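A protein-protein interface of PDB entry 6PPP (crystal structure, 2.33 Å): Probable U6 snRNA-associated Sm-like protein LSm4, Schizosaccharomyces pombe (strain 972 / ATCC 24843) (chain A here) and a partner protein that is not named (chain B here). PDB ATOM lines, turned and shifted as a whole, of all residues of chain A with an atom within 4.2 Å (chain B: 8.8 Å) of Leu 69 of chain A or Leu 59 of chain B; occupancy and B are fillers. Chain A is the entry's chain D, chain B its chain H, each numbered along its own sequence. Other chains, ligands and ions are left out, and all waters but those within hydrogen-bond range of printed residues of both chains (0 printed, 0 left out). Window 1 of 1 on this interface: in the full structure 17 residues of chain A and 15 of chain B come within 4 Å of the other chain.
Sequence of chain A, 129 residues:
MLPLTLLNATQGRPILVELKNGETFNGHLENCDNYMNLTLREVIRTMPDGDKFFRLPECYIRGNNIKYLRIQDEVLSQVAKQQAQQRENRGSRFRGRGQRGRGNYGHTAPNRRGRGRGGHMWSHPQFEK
N of Gly 62 of chain B is in hydrogen-bond range of OD1 of Asn 33 of chain B (2.7 Å).
The backbone NH (N) of Tyr 58 of chain B sits at hydrogen-bond distance from the backbone carbonyl oxygen (O) of Leu 36 of chain B.
The backbone NH (N) of Arg 70 of chain A lies within hydrogen-bond range of the backbone carbonyl oxygen (O) of Leu 16 of chain A.
The side-chain carboxylate of Asp 29 of chain B is in hydrogen-bond range of the side-chain amide nitrogen of Asn 33 of chain B (3.1 Å).
O of Gly 27 of chain B is in hydrogen-bond range of N of Ile 35 of chain B, 2.9 Å away.
O of Ser 39 of chain B is in hydrogen-bond range of N of Leu 55 of chain B (2.9 Å).
Printed residues of chain B within 4 Å of Tyr 68 of chain A: Tyr 58 (3.0 Å) and Leu 59 (3.4 Å).
Printed residues of chain B within 4 Å of Arg 70 of chain A: Leu 55 (3.0 Å), Val 57 (3.5 Å) and Tyr 58 (3.3 Å).
Printed residues of chain A within 4 Å of Ile 35 of chain B: Pro 3.
Leu 59 of chain B touches four residues of chain A.
The nearest residue of chain B that does not touch Leu 69 of chain A is Val 57 of chain B (4.1 Å).
The nearest printed residue of chain A that does not touch Leu 59 of chain B is Arg 70 of chain A (4.9 Å).
The nearest printed residue of chain A that does not touch Arg 61 of chain B is Tyr 68 of chain A (4.6 Å).
The side-chain sulfur of Met 36 of chain A sits at hydrogen-bond distance from the guanidinium group of Arg 61 of chain B (3.1 Å).
The backbone NH (N) of Leu 69 of chain A lies within hydrogen-bond range of the backbone carbonyl oxygen (O) of Leu 59 of chain B (2.7 Å).
The backbone carbonyl oxygen (O) of Leu 55 of chain B is in hydrogen-bond range of the guanidinium group (NE) of Arg 70 of chain A (3.0 Å).
Of the 22 printed residues of chain B, 9 touch a printed residue of chain A.
Hydrophobic or aromatic side chains of chain B within 4 Å of the printed part of chain A: Ile 35, Tyr 58 and Leu 59.
Among the printed residues, merely in contact across the chains: Tyr 68 of chain A with Tyr 58 of chain B, Met 36 of chain A with Leu 59 of chain B, Ile 66 of chain A with Arg 61 of chain B, Pro 3 of chain A with Leu 59 of chain B, Pro 3 of chain A with Asn 33 of chain B, Pro 3 of chain A with Asp 29 of chain B, Arg 70 of chain A with Tyr 58 of chain B, Tyr 68 of chain A with Leu 59 of chain B, Pro 3 of chain A with Phe 28 of chain B, Arg 70 of chain A with Val 57 of chain B, Pro 3 of chain A with Ile 35 of chain B and Leu 69 of chain A with Tyr 58 of chain B.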
ATOM      1  N   PRO A   3     -15.884  19.227 -14.178  1.00  0.00           N
ATOM      2  CA  PRO A   3     -16.250  17.826 -14.415  1.00  0.00           C
ATOM      3  C   PRO A   3     -17.470  17.684 -15.291  1.00  0.00           C
ATOM      4  O   PRO A   3     -17.495  16.794 -16.150  1.00  0.00           O
ATOM      5  CB  PRO A   3     -16.483  17.286 -13.004  1.00  0.00           C
ATOM      6  CG  PRO A   3     -15.598  18.166 -12.127  1.00  0.00           C
ATOM      7  CD  PRO A   3     -15.681  19.531 -12.749  1.00  0.00           C
ATOM      8  N   LEU A   7     -17.999  15.661 -18.818  1.00  0.00           N
ATOM      9  CA  LEU A   7     -19.035  14.642 -18.986  1.00  0.00           C
ATOM     10  C   LEU A   7     -19.938  14.996 -20.164  1.00  0.00           C
ATOM     11  O   LEU A   7     -20.359  14.119 -20.926  1.00  0.00           O
ATOM     12  CB  LEU A   7     -19.856  14.459 -17.713  1.00  0.00           C
ATOM     13  CG  LEU A   7     -20.943  13.405 -17.964  1.00  0.00           C
ATOM     14  CD1 LEU A   7     -20.467  12.046 -17.541  1.00  0.00           C
ATOM     15  CD2 LEU A   7     -22.211  13.751 -17.227  1.00  0.00           C
ATOM     16  N   ILE A  15     -17.881   5.218 -22.513  1.00  0.00           N
ATOM     17  CA  ILE A  15     -17.797   5.594 -21.113  1.00  0.00           C
ATOM     18  C   ILE A  15     -17.932   4.311 -20.312  1.00  0.00           C
ATOM     19  O   ILE A  15     -18.630   3.367 -20.718  1.00  0.00           O
ATOM     20  CB  ILE A  15     -18.910   6.594 -20.734  1.00  0.00           C
ATOM     21  CG1 ILE A  15     -18.630   7.238 -19.386  1.00  0.00           C
ATOM     22  CG2 ILE A  15     -20.265   5.894 -20.675  1.00  0.00           C
ATOM     23  CD1 ILE A  15     -19.626   8.318 -19.047  1.00  0.00           C
ATOM     24  N   LEU A  16     -17.247   4.271 -19.171  1.00  0.00           N
ATOM     25  CA  LEU A  16     -17.418   3.190 -18.217  1.00  0.00           C
ATOM     26  C   LEU A  16     -17.921   3.813 -16.931  1.00  0.00           C
ATOM     27  O   LEU A  16     -17.343   4.793 -16.455  1.00  0.00           O
ATOM     28  CB  LEU A  16     -16.097   2.441 -18.001  1.00  0.00           C
ATOM     29  CG  LEU A  16     -15.988   1.229 -17.068  1.00  0.00           C
ATOM     30  CD1 LEU A  16     -14.974   0.223 -17.619  1.00  0.00           C
ATOM     31  CD2 LEU A  16     -15.582   1.666 -15.672  1.00  0.00           C
ATOM     32  N   MET A  36     -25.925  14.634 -13.073  1.00  0.00           N
ATOM     33  CA  MET A  36     -25.142  13.482 -13.470  1.00  0.00           C
ATOM     34  C   MET A  36     -25.993  12.261 -13.775  1.00  0.00           C
ATOM     35  O   MET A  36     -25.450  11.148 -13.832  1.00  0.00           O
ATOM     36  CB  MET A  36     -24.135  13.096 -12.390  1.00  0.00           C
ATOM     37  CG  MET A  36     -22.887  12.491 -12.884  1.00  0.00           C
ATOM     38  SD  MET A  36     -21.754  12.562 -11.515  1.00  0.00           S
ATOM     39  CE  MET A  36     -20.271  12.655 -12.459  1.00  0.00           C
ATOM     40  N   LEU A  38     -27.503   9.757 -16.286  1.00  0.00           N
ATOM     41  CA  LEU A  38     -26.978   9.350 -17.588  1.00  0.00           C
ATOM     42  C   LEU A  38     -27.938   8.446 -18.356  1.00  0.00           C
ATOM     43  O   LEU A  38     -28.636   7.626 -17.756  1.00  0.00           O
ATOM     44  CB  LEU A  38     -25.624   8.618 -17.433  1.00  0.00           C
ATOM     45  CG  LEU A  38     -24.472   9.195 -16.601  1.00  0.00           C
ATOM     46  CD1 LEU A  38     -23.340   8.196 -16.569  1.00  0.00           C
ATOM     47  CD2 LEU A  38     -23.984  10.503 -17.183  1.00  0.00           C
ATOM     48  N   ILE A  66     -23.792   6.913  -8.721  1.00  0.00           N
ATOM     49  CA  ILE A  66     -22.530   6.673  -9.411  1.00  0.00           C
ATOM     50  C   ILE A  66     -21.386   6.866  -8.429  1.00  0.00           C
ATOM     51  O   ILE A  66     -21.345   7.830  -7.662  1.00  0.00           O
ATOM     52  CB  ILE A  66     -22.345   7.570 -10.643  1.00  0.00           C
ATOM     53  CG1 ILE A  66     -23.534   7.510 -11.603  1.00  0.00           C
ATOM     54  CG2 ILE A  66     -21.149   7.083 -11.386  1.00  0.00           C
ATOM     55  CD1 ILE A  66     -23.242   8.205 -12.915  1.00  0.00           C
ATOM     56  N   TYR A  68     -17.959   6.372  -9.896  1.00  0.00           N
ATOM     57  CA  TYR A  68     -17.031   7.094 -10.765  1.00  0.00           C
ATOM     58  C   TYR A  68     -17.293   6.772 -12.234  1.00  0.00           C
ATOM     59  O   TYR A  68     -18.005   5.816 -12.574  1.00  0.00           O
ATOM     60  CB  TYR A  68     -15.573   6.718 -10.417  1.00  0.00           C
ATOM     61  CG  TYR A  68     -15.280   5.277 -10.802  1.00  0.00           C
ATOM     62  CD1 TYR A  68     -15.264   4.257  -9.855  1.00  0.00           C
ATOM     63  CD2 TYR A  68     -15.067   4.928 -12.137  1.00  0.00           C
ATOM     64  CE1 TYR A  68     -15.032   2.923 -10.247  1.00  0.00           C
ATOM     65  CE2 TYR A  68     -14.862   3.627 -12.531  1.00  0.00           C
ATOM     66  CZ  TYR A  68     -14.833   2.629 -11.602  1.00  0.00           C
ATOM     67  OH  TYR A  68     -14.603   1.352 -12.068  1.00  0.00           O
ATOM     68  N   LEU A  69     -16.731   7.613 -13.106  1.00  0.00           N
ATOM     69  CA  LEU A  69     -16.768   7.414 -14.552  1.00  0.00           C
ATOM     70  C   LEU A  69     -15.356   7.424 -15.158  1.00  0.00           C
ATOM     71  O   LEU A  69     -14.477   8.182 -14.722  1.00  0.00           O
ATOM     72  CB  LEU A  69     -17.687   8.435 -15.248  1.00  0.00           C
ATOM     73  CG  LEU A  69     -19.166   8.444 -14.826  1.00  0.00           C
ATOM     74  CD1 LEU A  69     -19.385   9.044 -13.452  1.00  0.00           C
ATOM     75  CD2 LEU A  69     -19.999   9.202 -15.820  1.00  0.00           C
ATOM     76  N   ARG A  70     -15.158   6.608 -16.195  1.00  0.00           N
ATOM     77  CA  ARG A  70     -13.919   6.550 -16.966  1.00  0.00           C
ATOM     78  C   ARG A  70     -14.238   6.995 -18.380  1.00  0.00           C
ATOM     79  O   ARG A  70     -15.211   6.511 -18.976  1.00  0.00           O
ATOM     80  CB  ARG A  70     -13.299   5.143 -17.010  1.00  0.00           C
ATOM     81  CG  ARG A  70     -12.657   4.684 -15.716  1.00  0.00           C
ATOM     82  CD  ARG A  70     -11.898   3.347 -15.820  1.00  0.00           C
ATOM     83  NE  ARG A  70     -10.892   3.319 -16.878  1.00  0.00           N
ATOM     84  CZ  ARG A  70     -10.102   2.274 -17.146  1.00  0.00           C
ATOM     85  NH1 ARG A  70     -10.185   1.157 -16.426  1.00  0.00           N
ATOM     86  NH2 ARG A  70      -9.215   2.343 -18.135  1.00  0.00           N
ATOM     87  N   THR B  15     -11.403   7.436  -1.466  1.00  0.00           N
ATOM     88  CA  THR B  15     -12.826   7.407  -1.746  1.00  0.00           C
ATOM     89  C   THR B  15     -13.612   6.794  -0.603  1.00  0.00           C
ATOM     90  O   THR B  15     -13.078   6.038   0.213  1.00  0.00           O
ATOM     91  CB  THR B  15     -13.059   6.590  -3.015  1.00  0.00           C
ATOM     92  OG1 THR B  15     -12.256   5.400  -2.962  1.00  0.00           O
ATOM     93  CG2 THR B  15     -12.655   7.446  -4.214  1.00  0.00           C
ATOM     94  N   VAL B  21      -6.767   6.386  -5.488  1.00  0.00           N
ATOM     95  CA  VAL B  21      -6.475   6.588  -6.903  1.00  0.00           C
ATOM     96  C   VAL B  21      -5.714   7.888  -7.035  1.00  0.00           C
ATOM     97  O   VAL B  21      -6.049   8.876  -6.385  1.00  0.00           O
ATOM     98  CB  VAL B  21      -7.735   6.596  -7.805  1.00  0.00           C
ATOM     99  CG1 VAL B  21      -8.706   5.500  -7.429  1.00  0.00           C
ATOM    100  CG2 VAL B  21      -8.437   7.892  -7.758  1.00  0.00           C
ATOM    101  N   GLY B  27      -9.661  19.193 -12.978  1.00  0.00           N
ATOM    102  CA  GLY B  27     -10.754  20.091 -12.660  1.00  0.00           C
ATOM    103  C   GLY B  27     -11.600  19.505 -11.552  1.00  0.00           C
ATOM    104  O   GLY B  27     -11.529  18.310 -11.256  1.00  0.00           O
ATOM    105  N   PHE B  28     -12.402  20.378 -10.949  1.00  0.00           N
ATOM    106  CA  PHE B  28     -13.317  20.014  -9.876  1.00  0.00           C
ATOM    107  C   PHE B  28     -14.480  20.997  -9.902  1.00  0.00           C
ATOM    108  O   PHE B  28     -14.441  21.999 -10.617  1.00  0.00           O
ATOM    109  CB  PHE B  28     -12.622  20.056  -8.507  1.00  0.00           C
ATOM    110  CG  PHE B  28     -12.186  21.453  -8.092  1.00  0.00           C
ATOM    111  CD1 PHE B  28     -10.919  21.927  -8.426  1.00  0.00           C
ATOM    112  CD2 PHE B  28     -13.046  22.296  -7.398  1.00  0.00           C
ATOM    113  CE1 PHE B  28     -10.506  23.202  -8.067  1.00  0.00           C
ATOM    114  CE2 PHE B  28     -12.634  23.588  -7.028  1.00  0.00           C
ATOM    115  CZ  PHE B  28     -11.365  24.041  -7.366  1.00  0.00           C
ATOM    116  N   ASP B  29     -15.524  20.714  -9.113  1.00  0.00           N
ATOM    117  CA  ASP B  29     -16.608  21.673  -8.929  1.00  0.00           C
ATOM    118  C   ASP B  29     -17.051  21.647  -7.479  1.00  0.00           C
ATOM    119  O   ASP B  29     -16.539  20.864  -6.682  1.00  0.00           O
ATOM    120  CB  ASP B  29     -17.784  21.385  -9.866  1.00  0.00           C
ATOM    121  CG  ASP B  29     -18.184  19.957  -9.848  1.00  0.00           C
ATOM    122  OD1 ASP B  29     -18.209  19.356  -8.749  1.00  0.00           O
ATOM    123  OD2 ASP B  29     -18.456  19.421 -10.943  1.00  0.00           O
ATOM    124  N   THR B  32     -17.373  18.676  -5.306  1.00  0.00           N
ATOM    125  CA  THR B  32     -16.115  17.912  -5.281  1.00  0.00           C
ATOM    126  C   THR B  32     -16.044  16.788  -6.319  1.00  0.00           C
ATOM    127  O   THR B  32     -15.238  15.867  -6.153  1.00  0.00           O
ATOM    128  CB  THR B  32     -15.696  17.393  -3.886  1.00  0.00           C
ATOM    129  OG1 THR B  32     -16.813  16.926  -3.130  1.00  0.00           O
ATOM    130  CG2 THR B  32     -15.027  18.498  -3.109  1.00  0.00           C
ATOM    131  N   ASN B  33     -16.905  16.751  -7.340  1.00  0.00           N
ATOM    132  CA  ASN B  33     -16.573  15.939  -8.522  1.00  0.00           C
ATOM    133  C   ASN B  33     -15.164  16.268  -9.017  1.00  0.00           C
ATOM    134  O   ASN B  33     -14.769  17.435  -9.045  1.00  0.00           O
ATOM    135  CB  ASN B  33     -17.543  16.221  -9.678  1.00  0.00           C
ATOM    136  CG  ASN B  33     -18.982  16.024  -9.306  1.00  0.00           C
ATOM    137  OD1 ASN B  33     -19.315  15.136  -8.511  1.00  0.00           O
ATOM    138  ND2 ASN B  33     -19.856  16.858  -9.875  1.00  0.00           N
ATOM    139  N   LEU B  34     -14.421  15.267  -9.487  1.00  0.00           N
ATOM    140  CA  LEU B  34     -13.057  15.542  -9.930  1.00  0.00           C
ATOM    141  C   LEU B  34     -12.742  14.906 -11.289  1.00  0.00           C
ATOM    142  O   LEU B  34     -13.164  13.779 -11.590  1.00  0.00           O
ATOM    143  CB  LEU B  34     -12.035  15.041  -8.885  1.00  0.00           C
ATOM    144  CG  LEU B  34     -12.235  15.290  -7.384  1.00  0.00           C
ATOM    145  CD1 LEU B  34     -11.330  14.360  -6.607  1.00  0.00           C
ATOM    146  CD2 LEU B  34     -11.922  16.712  -6.986  1.00  0.00           C
ATOM    147  N   ILE B  35     -11.859  15.570 -12.038  1.00  0.00           N
ATOM    148  CA  ILE B  35     -11.212  14.982 -13.207  1.00  0.00           C
ATOM    149  C   ILE B  35      -9.758  14.780 -12.837  1.00  0.00           C
ATOM    150  O   ILE B  35      -9.056  15.735 -12.475  1.00  0.00           O
ATOM    151  CB  ILE B  35     -11.305  15.891 -14.446  1.00  0.00           C
ATOM    152  CG1 ILE B  35     -12.749  16.264 -14.754  1.00  0.00           C
ATOM    153  CG2 ILE B  35     -10.700  15.212 -15.636  1.00  0.00           C
ATOM    154  CD1 ILE B  35     -12.892  17.567 -15.450  1.00  0.00           C
ATOM    155  N   LEU B  36      -9.315  13.542 -12.945  1.00  0.00           N
ATOM    156  CA  LEU B  36      -7.926  13.164 -12.848  1.00  0.00           C
ATOM    157  C   LEU B  36      -7.514  12.607 -14.189  1.00  0.00           C
ATOM    158  O   LEU B  36      -8.256  11.833 -14.808  1.00  0.00           O
ATOM    159  CB  LEU B  36      -7.691  12.136 -11.750  1.00  0.00           C
ATOM    160  CG  LEU B  36      -8.321  12.518 -10.414  1.00  0.00           C
ATOM    161  CD1 LEU B  36      -8.171  11.413  -9.401  1.00  0.00           C
ATOM    162  CD2 LEU B  36      -7.676  13.796  -9.905  1.00  0.00           C
ATOM    163  N   SER B  37      -6.337  12.971 -14.639  1.00  0.00           N
ATOM    164  CA  SER B  37      -5.866  12.353 -15.853  1.00  0.00           C
ATOM    165  C   SER B  37      -4.605  11.563 -15.553  1.00  0.00           C
ATOM    166  O   SER B  37      -3.992  11.690 -14.485  1.00  0.00           O
ATOM    167  CB  SER B  37      -5.599  13.420 -16.915  1.00  0.00           C
ATOM    168  OG  SER B  37      -4.531  13.016 -17.744  1.00  0.00           O
ATOM    169  N   SER B  39      -4.426   8.691 -14.449  1.00  0.00           N
ATOM    170  CA  SER B  39      -4.589   8.213 -13.098  1.00  0.00           C
ATOM    171  C   SER B  39      -4.409   6.698 -13.006  1.00  0.00           C
ATOM    172  O   SER B  39      -4.539   5.957 -13.981  1.00  0.00           O
ATOM    173  CB  SER B  39      -6.003   8.537 -12.635  1.00  0.00           C
ATOM    174  OG  SER B  39      -6.855   7.479 -13.064  1.00  0.00           O
ATOM    175  N   LEU B  55      -5.830   3.463 -14.782  1.00  0.00           N
ATOM    176  CA  LEU B  55      -7.223   3.892 -14.928  1.00  0.00           C
ATOM    177  C   LEU B  55      -7.497   4.977 -15.975  1.00  0.00           C
ATOM    178  O   LEU B  55      -8.673   5.223 -16.283  1.00  0.00           O
ATOM    179  CB  LEU B  55      -7.745   4.397 -13.571  1.00  0.00           C
ATOM    180  CG  LEU B  55      -7.617   3.323 -12.493  1.00  0.00           C
ATOM    181  CD1 LEU B  55      -7.947   3.914 -11.149  1.00  0.00           C
ATOM    182  CD2 LEU B  55      -8.519   2.146 -12.826  1.00  0.00           C
ATOM    183  N   GLY B  56      -6.475   5.670 -16.481  1.00  0.00           N
ATOM    184  CA  GLY B  56      -6.682   6.678 -17.520  1.00  0.00           C
ATOM    185  C   GLY B  56      -7.323   7.945 -16.971  1.00  0.00           C
ATOM    186  O   GLY B  56      -6.994   8.401 -15.869  1.00  0.00           O
ATOM    187  N   VAL B  57      -8.304   8.487 -17.698  1.00  0.00           N
ATOM    188  CA  VAL B  57      -9.013   9.678 -17.239  1.00  0.00           C
ATOM    189  C   VAL B  57     -10.167   9.222 -16.359  1.00  0.00           C
ATOM    190  O   VAL B  57     -10.936   8.323 -16.732  1.00  0.00           O
ATOM    191  CB  VAL B  57      -9.494  10.526 -18.423  1.00  0.00           C
ATOM    192  CG1 VAL B  57     -10.196  11.787 -17.947  1.00  0.00           C
ATOM    193  CG2 VAL B  57      -8.307  10.883 -19.281  1.00  0.00           C
ATOM    194  N   TYR B  58     -10.271   9.835 -15.180  1.00  0.00           N
ATOM    195  CA  TYR B  58     -11.137   9.364 -14.109  1.00  0.00           C
ATOM    196  C   TYR B  58     -11.949  10.535 -13.608  1.00  0.00           C
ATOM    197  O   TYR B  58     -11.383  11.485 -13.058  1.00  0.00           O
ATOM    198  CB  TYR B  58     -10.308   8.780 -12.973  1.00  0.00           C
ATOM    199  CG  TYR B  58     -10.834   7.464 -12.389  1.00  0.00           C
ATOM    200  CD1 TYR B  58     -10.945   6.325 -13.184  1.00  0.00           C
ATOM    201  CD2 TYR B  58     -11.202   7.366 -11.031  1.00  0.00           C
ATOM    202  CE1 TYR B  58     -11.413   5.136 -12.665  1.00  0.00           C
ATOM    203  CE2 TYR B  58     -11.676   6.181 -10.504  1.00  0.00           C
ATOM    204  CZ  TYR B  58     -11.782   5.071 -11.331  1.00  0.00           C
ATOM    205  OH  TYR B  58     -12.245   3.877 -10.831  1.00  0.00           O
ATOM    206  N   LEU B  59     -13.260  10.485 -13.821  1.00  0.00           N
ATOM    207  CA  LEU B  59     -14.184  11.458 -13.246  1.00  0.00           C
ATOM    208  C   LEU B  59     -14.839  10.850 -12.006  1.00  0.00           C
ATOM    209  O   LEU B  59     -15.426   9.762 -12.094  1.00  0.00           O
ATOM    210  CB  LEU B  59     -15.222  11.915 -14.266  1.00  0.00           C
ATOM    211  CG  LEU B  59     -16.126  12.930 -13.572  1.00  0.00           C
ATOM    212  CD1 LEU B  59     -16.130  14.297 -14.234  1.00  0.00           C
ATOM    213  CD2 LEU B  59     -17.483  12.380 -13.563  1.00  0.00           C
ATOM    214  N   LEU B  60     -14.632  11.486 -10.843  1.00  0.00           N
ATOM    215  CA  LEU B  60     -15.094  10.996  -9.537  1.00  0.00           C
ATOM    216  C   LEU B  60     -16.253  11.840  -9.038  1.00  0.00           C
ATOM    217  O   LEU B  60     -16.177  13.074  -9.043  1.00  0.00           O
ATOM    218  CB  LEU B  60     -13.986  11.004  -8.481  1.00  0.00           C
ATOM    219  CG  LEU B  60     -12.902   9.917  -8.643  1.00  0.00           C
ATOM    220  CD1 LEU B  60     -11.517  10.543  -8.882  1.00  0.00           C
ATOM    221  CD2 LEU B  60     -12.853   8.991  -7.480  1.00  0.00           C
ATOM    222  N   ARG B  61     -17.339  11.180  -8.654  1.00  0.00           N
ATOM    223  CA  ARG B  61     -18.500  11.894  -8.131  1.00  0.00           C
ATOM    224  C   ARG B  61     -18.258  12.339  -6.686  1.00  0.00           C
ATOM    225  O   ARG B  61     -17.812  11.560  -5.852  1.00  0.00           O
ATOM    226  CB  ARG B  61     -19.751  11.012  -8.237  1.00  0.00           C
ATOM    227  CG  ARG B  61     -21.055  11.728  -7.890  1.00  0.00           C
ATOM    228  CD  ARG B  61     -22.123  10.747  -7.347  1.00  0.00           C
ATOM    229  NE  ARG B  61     -23.391  11.440  -7.063  1.00  0.00           N
ATOM    230  CZ  ARG B  61     -24.156  12.041  -7.980  1.00  0.00           C
ATOM    231  NH1 ARG B  61     -23.807  12.035  -9.262  1.00  0.00           N
ATOM    232  NH2 ARG B  61     -25.289  12.640  -7.626  1.00  0.00           N
ATOM    233  N   GLY B  62     -18.568  13.588  -6.384  1.00  0.00           N
ATOM    234  CA  GLY B  62     -18.152  14.143  -5.105  1.00  0.00           C
ATOM    235  C   GLY B  62     -18.720  13.417  -3.892  1.00  0.00           C
ATOM    236  O   GLY B  62     -18.033  13.269  -2.869  1.00  0.00           O
ATOM    237  N   ASN B  64     -18.688  10.567  -3.274  1.00  0.00           N
ATOM    238  CA  ASN B  64     -17.833   9.433  -2.952  1.00  0.00           C
ATOM    239  C   ASN B  64     -16.414   9.817  -2.539  1.00  0.00           C
ATOM    240  O   ASN B  64     -15.569   8.931  -2.379  1.00  0.00           O
ATOM    241  CB  ASN B  64     -17.774   8.439  -4.107  1.00  0.00           C
ATOM    242  CG  ASN B  64     -17.556   7.032  -3.609  1.00  0.00           C
ATOM    243  OD1 ASN B  64     -16.468   6.466  -3.756  1.00  0.00           O
ATOM    244  ND2 ASN B  64     -18.590   6.462  -2.975  1.00  0.00           N
ATOM    245  N   VAL B  65     -16.109  11.103  -2.453  1.00  0.00           N
ATOM    246  CA  VAL B  65     -14.768  11.585  -2.139  1.00  0.00           C
ATOM    247  C   VAL B  65     -14.634  11.854  -0.633  1.00  0.00           C
ATOM    248  O   VAL B  65     -15.397  12.638  -0.061  1.00  0.00           O
ATOM    249  CB  VAL B  65     -14.481  12.862  -2.946  1.00  0.00           C
ATOM    250  CG1 VAL B  65     -13.022  13.295  -2.838  1.00  0.00           C
ATOM    251  CG2 VAL B  65     -14.919  12.663  -4.403  1.00  0.00           C
